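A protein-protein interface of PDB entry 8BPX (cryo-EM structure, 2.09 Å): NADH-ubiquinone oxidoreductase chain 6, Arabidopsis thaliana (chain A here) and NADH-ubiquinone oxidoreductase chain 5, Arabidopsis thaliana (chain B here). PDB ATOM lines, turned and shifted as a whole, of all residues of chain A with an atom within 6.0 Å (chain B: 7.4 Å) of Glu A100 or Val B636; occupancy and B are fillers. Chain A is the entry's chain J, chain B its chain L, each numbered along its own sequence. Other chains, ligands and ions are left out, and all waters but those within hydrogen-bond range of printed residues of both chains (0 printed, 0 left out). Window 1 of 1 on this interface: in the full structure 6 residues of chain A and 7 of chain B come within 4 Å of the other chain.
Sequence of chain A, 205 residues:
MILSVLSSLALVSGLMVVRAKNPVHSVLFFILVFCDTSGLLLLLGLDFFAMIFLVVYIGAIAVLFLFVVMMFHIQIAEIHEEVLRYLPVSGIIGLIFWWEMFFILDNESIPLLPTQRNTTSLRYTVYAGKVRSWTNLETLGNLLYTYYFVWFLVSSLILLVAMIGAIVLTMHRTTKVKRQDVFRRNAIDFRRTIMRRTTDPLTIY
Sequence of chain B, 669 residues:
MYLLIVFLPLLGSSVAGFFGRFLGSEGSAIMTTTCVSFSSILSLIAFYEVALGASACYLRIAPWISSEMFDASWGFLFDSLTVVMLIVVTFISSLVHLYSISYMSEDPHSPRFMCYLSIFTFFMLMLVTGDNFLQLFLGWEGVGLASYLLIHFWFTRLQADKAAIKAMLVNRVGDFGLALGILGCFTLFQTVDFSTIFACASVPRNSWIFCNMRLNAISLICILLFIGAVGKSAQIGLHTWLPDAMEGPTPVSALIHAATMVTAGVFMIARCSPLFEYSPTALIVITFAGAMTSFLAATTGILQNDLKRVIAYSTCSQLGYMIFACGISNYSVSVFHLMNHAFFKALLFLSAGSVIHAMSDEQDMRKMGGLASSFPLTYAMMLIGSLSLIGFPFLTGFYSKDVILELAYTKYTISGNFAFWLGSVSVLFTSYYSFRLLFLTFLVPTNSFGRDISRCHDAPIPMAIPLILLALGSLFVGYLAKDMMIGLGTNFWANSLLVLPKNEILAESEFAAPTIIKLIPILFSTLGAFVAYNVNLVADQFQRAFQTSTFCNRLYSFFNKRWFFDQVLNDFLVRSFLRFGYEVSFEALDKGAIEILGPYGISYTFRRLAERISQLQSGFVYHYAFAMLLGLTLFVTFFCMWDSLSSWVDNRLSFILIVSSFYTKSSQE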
ATOM      1  N   LEU A  95      24.734  18.192  18.509  1.00  0.00           N
ATOM      2  CA  LEU A  95      24.630  19.343  17.567  1.00  0.00           C
ATOM      3  C   LEU A  95      23.722  20.428  18.161  1.00  0.00           C
ATOM      4  O   LEU A  95      24.172  21.566  18.243  1.00  0.00           O
ATOM      5  CB  LEU A  95      24.096  18.895  16.207  1.00  0.00           C
ATOM      6  CG  LEU A  95      23.899  20.002  15.174  1.00  0.00           C
ATOM      7  CD1 LEU A  95      25.090  20.076  14.230  1.00  0.00           C
ATOM      8  CD2 LEU A  95      22.610  19.790  14.393  1.00  0.00           C
ATOM      9  N   ILE A  96      22.485  20.095  18.522  1.00  0.00           N
ATOM     10  CA  ILE A  96      21.554  21.083  19.067  1.00  0.00           C
ATOM     11  C   ILE A  96      22.180  21.800  20.251  1.00  0.00           C
ATOM     12  O   ILE A  96      22.172  23.034  20.331  1.00  0.00           O
ATOM     13  CB  ILE A  96      20.223  20.419  19.459  1.00  0.00           C
ATOM     14  CG1 ILE A  96      19.543  19.792  18.240  1.00  0.00           C
ATOM     15  CG2 ILE A  96      19.319  21.414  20.168  1.00  0.00           C
ATOM     16  CD1 ILE A  96      18.236  19.108  18.563  1.00  0.00           C
ATOM     17  N   PHE A  97      22.736  21.034  21.187  1.00  0.00           N
ATOM     18  CA  PHE A  97      23.467  21.641  22.288  1.00  0.00           C
ATOM     19  C   PHE A  97      24.662  22.430  21.771  1.00  0.00           C
ATOM     20  O   PHE A  97      24.940  23.530  22.251  1.00  0.00           O
ATOM     21  CB  PHE A  97      23.914  20.567  23.278  1.00  0.00           C
ATOM     22  CG  PHE A  97      22.912  20.286  24.363  1.00  0.00           C
ATOM     23  CD1 PHE A  97      21.917  19.340  24.173  1.00  0.00           C
ATOM     24  CD2 PHE A  97      22.966  20.957  25.573  1.00  0.00           C
ATOM     25  CE1 PHE A  97      20.993  19.069  25.165  1.00  0.00           C
ATOM     26  CE2 PHE A  97      22.042  20.692  26.572  1.00  0.00           C
ATOM     27  CZ  PHE A  97      21.054  19.746  26.364  1.00  0.00           C
ATOM     28  N   TRP A  98      25.366  21.896  20.772  1.00  0.00           N
ATOM     29  CA  TRP A  98      26.500  22.629  20.217  1.00  0.00           C
ATOM     30  C   TRP A  98      26.063  23.956  19.604  1.00  0.00           C
ATOM     31  O   TRP A  98      26.627  25.007  19.922  1.00  0.00           O
ATOM     32  CB  TRP A  98      27.219  21.785  19.174  1.00  0.00           C
ATOM     33  CG  TRP A  98      28.358  22.503  18.536  1.00  0.00           C
ATOM     34  CD1 TRP A  98      29.588  22.744  19.076  1.00  0.00           C
ATOM     35  CD2 TRP A  98      28.363  23.107  17.240  1.00  0.00           C
ATOM     36  NE1 TRP A  98      30.363  23.445  18.188  1.00  0.00           N
ATOM     37  CE2 TRP A  98      29.633  23.683  17.053  1.00  0.00           C
ATOM     38  CE3 TRP A  98      27.417  23.213  16.217  1.00  0.00           C
ATOM     39  CZ2 TRP A  98      29.984  24.354  15.885  1.00  0.00           C
ATOM     40  CZ3 TRP A  98      27.766  23.880  15.058  1.00  0.00           C
ATOM     41  CH2 TRP A  98      29.039  24.441  14.902  1.00  0.00           C
ATOM     42  N   TRP A  99      25.052  23.924  18.733  1.00  0.00           N
ATOM     43  CA  TRP A  99      24.629  25.130  18.025  1.00  0.00           C
ATOM     44  C   TRP A  99      24.062  26.177  18.971  1.00  0.00           C
ATOM     45  O   TRP A  99      24.210  27.381  18.735  1.00  0.00           O
ATOM     46  CB  TRP A  99      23.594  24.773  16.960  1.00  0.00           C
ATOM     47  CG  TRP A  99      22.924  25.973  16.361  1.00  0.00           C
ATOM     48  CD1 TRP A  99      21.596  26.268  16.410  1.00  0.00           C
ATOM     49  CD2 TRP A  99      23.548  27.050  15.646  1.00  0.00           C
ATOM     50  NE1 TRP A  99      21.348  27.452  15.762  1.00  0.00           N
ATOM     51  CE2 TRP A  99      22.529  27.953  15.284  1.00  0.00           C
ATOM     52  CE3 TRP A  99      24.865  27.335  15.271  1.00  0.00           C
ATOM     53  CZ2 TRP A  99      22.784  29.121  14.568  1.00  0.00           C
ATOM     54  CZ3 TRP A  99      25.117  28.495  14.560  1.00  0.00           C
ATOM     55  CH2 TRP A  99      24.082  29.373  14.216  1.00  0.00           C
ATOM     56  N   GLU A 100      23.420  25.745  20.043  1.00  0.00           N
ATOM     57  CA  GLU A 100      22.802  26.686  20.959  1.00  0.00           C
ATOM     58  C   GLU A 100      23.760  27.197  22.016  1.00  0.00           C
ATOM     59  O   GLU A 100      23.723  28.378  22.368  1.00  0.00           O
ATOM     60  CB  GLU A 100      21.638  26.010  21.674  1.00  0.00           C
ATOM     61  CG  GLU A 100      20.860  26.958  22.503  1.00  0.00           C
ATOM     62  CD  GLU A 100      19.911  27.740  21.662  1.00  0.00           C
ATOM     63  OE1 GLU A 100      19.222  27.116  20.833  1.00  0.00           O
ATOM     64  OE2 GLU A 100      19.886  28.979  21.802  1.00  0.00           O
ATOM     65  N   MET A 101      24.613  26.337  22.509  1.00  0.00           N
ATOM     66  CA  MET A 101      25.157  26.484  23.841  1.00  0.00           C
ATOM     67  C   MET A 101      26.644  26.824  23.846  1.00  0.00           C
ATOM     68  O   MET A 101      27.139  27.361  24.837  1.00  0.00           O
ATOM     69  CB  MET A 101      24.847  25.195  24.620  1.00  0.00           C
ATOM     70  CG  MET A 101      25.706  24.866  25.738  1.00  0.00           C
ATOM     71  SD  MET A 101      24.802  25.243  27.254  1.00  0.00           S
ATOM     72  CE  MET A 101      23.496  24.007  27.286  1.00  0.00           C
ATOM     73  N   PHE A 102      27.367  26.531  22.762  1.00  0.00           N
ATOM     74  CA  PHE A 102      28.711  27.077  22.566  1.00  0.00           C
ATOM     75  C   PHE A 102      28.690  28.527  22.103  1.00  0.00           C
ATOM     76  O   PHE A 102      29.711  29.209  22.214  1.00  0.00           O
ATOM     77  CB  PHE A 102      29.492  26.249  21.543  1.00  0.00           C
ATOM     78  CG  PHE A 102      29.929  24.911  22.042  1.00  0.00           C
ATOM     79  CD1 PHE A 102      29.001  23.908  22.266  1.00  0.00           C
ATOM     80  CD2 PHE A 102      31.266  24.640  22.265  1.00  0.00           C
ATOM     81  CE1 PHE A 102      29.404  22.672  22.722  1.00  0.00           C
ATOM     82  CE2 PHE A 102      31.671  23.405  22.716  1.00  0.00           C
ATOM     83  CZ  PHE A 102      30.741  22.423  22.944  1.00  0.00           C
ATOM     84  N   PHE A 103      27.554  29.006  21.591  1.00  0.00           N
ATOM     85  CA  PHE A 103      27.449  30.338  21.002  1.00  0.00           C
ATOM     86  C   PHE A 103      26.476  31.232  21.755  1.00  0.00           C
ATOM     87  O   PHE A 103      26.087  32.282  21.233  1.00  0.00           O
ATOM     88  CB  PHE A 103      27.030  30.229  19.531  1.00  0.00           C
ATOM     89  CG  PHE A 103      27.868  29.268  18.735  1.00  0.00           C
ATOM     90  CD1 PHE A 103      29.170  29.587  18.389  1.00  0.00           C
ATOM     91  CD2 PHE A 103      27.360  28.036  18.356  1.00  0.00           C
ATOM     92  CE1 PHE A 103      29.948  28.701  17.664  1.00  0.00           C
ATOM     93  CE2 PHE A 103      28.133  27.147  17.634  1.00  0.00           C
ATOM     94  CZ  PHE A 103      29.430  27.479  17.290  1.00  0.00           C
ATOM     95  N   ILE A 104      26.076  30.844  22.967  1.00  0.00           N
ATOM     96  CA  ILE A 104      25.083  31.600  23.723  1.00  0.00           C
ATOM     97  C   ILE A 104      25.618  32.971  24.118  1.00  0.00           C
ATOM     98  O   ILE A 104      24.862  33.947  24.174  1.00  0.00           O
ATOM     99  CB  ILE A 104      24.632  30.773  24.944  1.00  0.00           C
ATOM    100  CG1 ILE A 104      23.695  31.563  25.853  1.00  0.00           C
ATOM    101  CG2 ILE A 104      25.816  30.292  25.720  1.00  0.00           C
ATOM    102  CD1 ILE A 104      22.698  30.697  26.576  1.00  0.00           C
ATOM    103  N   LEU B 630      15.722  14.242  26.842  1.00  0.00           N
ATOM    104  CA  LEU B 630      14.820  14.527  25.732  1.00  0.00           C
ATOM    105  C   LEU B 630      13.908  15.706  26.053  1.00  0.00           C
ATOM    106  O   LEU B 630      13.673  16.569  25.200  1.00  0.00           O
ATOM    107  CB  LEU B 630      13.999  13.285  25.400  1.00  0.00           C
ATOM    108  CG  LEU B 630      14.699  12.207  24.570  1.00  0.00           C
ATOM    109  CD1 LEU B 630      13.761  11.036  24.321  1.00  0.00           C
ATOM    110  CD2 LEU B 630      15.225  12.770  23.256  1.00  0.00           C
ATOM    111  N   GLY B 631      13.380  15.754  27.278  1.00  0.00           N
ATOM    112  CA  GLY B 631      12.558  16.885  27.672  1.00  0.00           C
ATOM    113  C   GLY B 631      13.327  18.192  27.670  1.00  0.00           C
ATOM    114  O   GLY B 631      12.810  19.227  27.245  1.00  0.00           O
ATOM    115  N   LEU B 632      14.572  18.162  28.149  1.00  0.00           N
ATOM    116  CA  LEU B 632      15.416  19.351  28.096  1.00  0.00           C
ATOM    117  C   LEU B 632      15.688  19.772  26.656  1.00  0.00           C
ATOM    118  O   LEU B 632      15.626  20.961  26.325  1.00  0.00           O
ATOM    119  CB  LEU B 632      16.723  19.093  28.842  1.00  0.00           C
ATOM    120  CG  LEU B 632      17.774  20.201  28.838  1.00  0.00           C
ATOM    121  CD1 LEU B 632      17.286  21.407  29.623  1.00  0.00           C
ATOM    122  CD2 LEU B 632      19.086  19.690  29.404  1.00  0.00           C
ATOM    123  N   THR B 633      15.982  18.806  25.782  1.00  0.00           N
ATOM    124  CA  THR B 633      16.221  19.119  24.376  1.00  0.00           C
ATOM    125  C   THR B 633      14.975  19.691  23.715  1.00  0.00           C
ATOM    126  O   THR B 633      15.055  20.662  22.955  1.00  0.00           O
ATOM    127  CB  THR B 633      16.693  17.867  23.636  1.00  0.00           C
ATOM    128  OG1 THR B 633      17.831  17.318  24.309  1.00  0.00           O
ATOM    129  CG2 THR B 633      17.064  18.204  22.200  1.00  0.00           C
ATOM    130  N   LEU B 634      13.825  19.069  23.964  1.00  0.00           N
ATOM    131  CA  LEU B 634      12.527  19.585  23.473  1.00  0.00           C
ATOM    132  C   LEU B 634      12.348  21.041  23.927  1.00  0.00           C
ATOM    133  O   LEU B 634      11.980  21.871  23.081  1.00  0.00           O
ATOM    134  CB  LEU B 634      11.405  18.682  23.997  1.00  0.00           C
ATOM    135  CG  LEU B 634       9.991  19.245  23.870  1.00  0.00           C
ATOM    136  CD1 LEU B 634       9.489  19.130  22.439  1.00  0.00           C
ATOM    137  CD2 LEU B 634       9.042  18.545  24.829  1.00  0.00           C
ATOM    138  N   PHE B 635      12.604  21.329  25.203  1.00  0.00           N
ATOM    139  CA  PHE B 635      12.419  22.672  25.742  1.00  0.00           C
ATOM    140  C   PHE B 635      13.237  23.697  24.966  1.00  0.00           C
ATOM    141  O   PHE B 635      12.711  24.719  24.511  1.00  0.00           O
ATOM    142  CB  PHE B 635      12.810  22.696  27.218  1.00  0.00           C
ATOM    143  CG  PHE B 635      11.681  22.390  28.154  1.00  0.00           C
ATOM    144  CD1 PHE B 635      10.533  21.763  27.701  1.00  0.00           C
ATOM    145  CD2 PHE B 635      11.775  22.720  29.493  1.00  0.00           C
ATOM    146  CE1 PHE B 635       9.497  21.474  28.571  1.00  0.00           C
ATOM    147  CE2 PHE B 635      10.743  22.437  30.365  1.00  0.00           C
ATOM    148  CZ  PHE B 635       9.605  21.812  29.904  1.00  0.00           C
ATOM    149  N   VAL B 636      14.535  23.431  24.806  1.00  0.00           N
ATOM    150  CA  VAL B 636      15.406  24.346  24.073  1.00  0.00           C
ATOM    151  C   VAL B 636      14.942  24.477  22.629  1.00  0.00           C
ATOM    152  O   VAL B 636      14.848  25.583  22.085  1.00  0.00           O
ATOM    153  CB  VAL B 636      16.866  23.868  24.154  1.00  0.00           C
ATOM    154  CG1 VAL B 636      17.750  24.676  23.213  1.00  0.00           C
ATOM    155  CG2 VAL B 636      17.373  23.965  25.582  1.00  0.00           C
ATOM    156  N   THR B 637      14.626  23.348  21.995  1.00  0.00           N
ATOM    157  CA  THR B 637      14.302  23.359  20.573  1.00  0.00           C
ATOM    158  C   THR B 637      13.038  24.160  20.295  1.00  0.00           C
ATOM    159  O   THR B 637      13.039  25.071  19.459  1.00  0.00           O
ATOM    160  CB  THR B 637      14.157  21.928  20.057  1.00  0.00           C
ATOM    161  OG1 THR B 637      15.455  21.394  19.776  1.00  0.00           O
ATOM    162  CG2 THR B 637      13.318  21.898  18.787  1.00  0.00           C
ATOM    163  N   PHE B 638      11.949  23.852  20.997  1.00  0.00           N
ATOM    164  CA  PHE B 638      10.677  24.476  20.656  1.00  0.00           C
ATOM    165  C   PHE B 638      10.634  25.928  21.111  1.00  0.00           C
ATOM    166  O   PHE B 638      10.134  26.797  20.390  1.00  0.00           O
ATOM    167  CB  PHE B 638       9.513  23.676  21.249  1.00  0.00           C
ATOM    168  CG  PHE B 638       8.217  24.441  21.308  1.00  0.00           C
ATOM    169  CD1 PHE B 638       7.908  25.245  22.395  1.00  0.00           C
ATOM    170  CD2 PHE B 638       7.321  24.383  20.257  1.00  0.00           C
ATOM    171  CE1 PHE B 638       6.726  25.953  22.443  1.00  0.00           C
ATOM    172  CE2 PHE B 638       6.134  25.093  20.299  1.00  0.00           C
ATOM    173  CZ  PHE B 638       5.837  25.879  21.393  1.00  0.00           C
ATOM    174  N   PHE B 639      11.143  26.213  22.303  1.00  0.00           N
ATOM    175  CA  PHE B 639      10.907  27.509  22.926  1.00  0.00           C
ATOM    176  C   PHE B 639      11.963  28.556  22.608  1.00  0.00           C
ATOM    177  O   PHE B 639      11.769  29.723  22.959  1.00  0.00           O
ATOM    178  CB  PHE B 639      10.788  27.334  24.440  1.00  0.00           C
ATOM    179  CG  PHE B 639       9.372  27.258  24.918  1.00  0.00           C
ATOM    180  CD1 PHE B 639       8.846  26.066  25.375  1.00  0.00           C
ATOM    181  CD2 PHE B 639       8.571  28.385  24.934  1.00  0.00           C
ATOM    182  CE1 PHE B 639       7.545  25.985  25.811  1.00  0.00           C
ATOM    183  CE2 PHE B 639       7.270  28.311  25.385  1.00  0.00           C
ATOM    184  CZ  PHE B 639       6.759  27.109  25.824  1.00  0.00           C
ATOM    185  N   CYS B 640      13.077  28.188  21.977  1.00  0.00           N
ATOM    186  CA  CYS B 640      14.036  29.196  21.543  1.00  0.00           C
ATOM    187  C   CYS B 640      14.411  29.050  20.073  1.00  0.00           C
ATOM    188  O   CYS B 640      14.466  30.053  19.357  1.00  0.00           O
ATOM    189  CB  CYS B 640      15.273  29.132  22.451  1.00  0.00           C
ATOM    190  SG  CYS B 640      16.148  30.704  22.659  1.00  0.00           S
ATOM    191  N   MET B 641      14.651  27.830  19.594  1.00  0.00           N
ATOM    192  CA  MET B 641      14.927  27.556  18.177  1.00  0.00           C
ATOM    193  C   MET B 641      13.643  27.223  17.421  1.00  0.00           C
ATOM    194  O   MET B 641      13.451  26.137  16.871  1.00  0.00           O
ATOM    195  CB  MET B 641      15.978  26.462  18.044  1.00  0.00           C
ATOM    196  CG  MET B 641      17.406  26.900  18.362  1.00  0.00           C
ATOM    197  SD  MET B 641      17.710  28.680  18.134  1.00  0.00           S
ATOM    198  CE  MET B 641      17.594  29.379  19.769  1.00  0.00           C
ATOM    199  N   TRP B 642      12.672  28.132  17.498  1.00  0.00           N
ATOM    200  CA  TRP B 642      11.501  28.131  16.576  1.00  0.00           C
ATOM    201  C   TRP B 642      11.348  29.532  15.964  1.00  0.00           C
ATOM    202  O   TRP B 642      10.209  30.024  15.910  1.00  0.00           O
ATOM    203  CB  TRP B 642      10.248  27.700  17.359  1.00  0.00           C
ATOM    204  CG  TRP B 642       9.310  26.724  16.718  1.00  0.00           C
ATOM    205  CD1 TRP B 642       8.118  27.012  16.121  1.00  0.00           C
ATOM    206  CD2 TRP B 642       9.439  25.292  16.678  1.00  0.00           C
ATOM    207  NE1 TRP B 642       7.512  25.863  15.686  1.00  0.00           N
ATOM    208  CE2 TRP B 642       8.301  24.792  16.012  1.00  0.00           C
ATOM    209  CE3 TRP B 642      10.411  24.386  17.115  1.00  0.00           C
ATOM    210  CZ2 TRP B 642       8.110  23.432  15.774  1.00  0.00           C
ATOM    211  CZ3 TRP B 642      10.221  23.041  16.885  1.00  0.00           C
ATOM    212  CH2 TRP B 642       9.086  22.573  16.225  1.00  0.00           C
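The backbone carbonyl oxygen (O) of Thr B633 sits at hydrogen-bond distance from the side-chain hydroxyl (OG1) of Thr B637 (3.3 Å). N of Met B641 sits at hydrogen-bond distance from O of Val B636 (3.4 Å).
Glu A100 touches two residues of chain B. Val B636 touches just one residue of chain A: Glu A100. Printed residues of chain A within 4 Å of Leu B632: Phe A97. Of the printed residues of chain A, Met B641 touches Glu A100. Of the printed residues of chain A, Thr B633 touches Ile A96 (3.9 Å) and Phe A97 (3.7 Å). Printed residues of chain B within 4 Å of Ile A96: Thr B633 and Thr B637. Printed residues of chain A within 4 Å of Thr B637: Ile A96 (3.8 Å). Met A101 touches none of the printed residues of chain B. Leu A95 touches none of the printed residues of chain B. The nearest residue of chain A that does not touch Val B636 is Ile A96 (4.7 Å). The nearest printed residue of chain A that does not touch Leu B632 is Met A101 (6.5 Å).
Of the 13 printed residues of chain B, 5 touch a printed residue of chain A. Printed residues of chain B that touch a printed residue of chain A: Leu B632, Thr B633, Val B636, Thr B637 and Met B641. Printed residues of chain A that touch a printed residue of chain B: Ile A96, Phe A97 and Glu A100. Hydrophobic or aromatic side chains of chain A within 4 Å of the printed part of chain B: Ile A96 and Phe A97. Among the printed residues, 6 pairs touch across the chains. Among the printed residues, no Asp or Glu carboxylate lies within 4 Å of a Lys or Arg side-chain nitrogen of the other chain.
Among the printed residues, pairs that only touch across the chains: Ile A96 with Thr B633 (3.9 Å), Ile A96 with Thr B637 (3.8 Å), Phe A97 with Leu B632 (3.6 Å), Phe A97 with Thr B633 (3.7 Å) and Glu A100 with Val B636 (3.7 Å).
SD of Met B641 sits close to OE1 of Glu A100 (3.5 Å).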
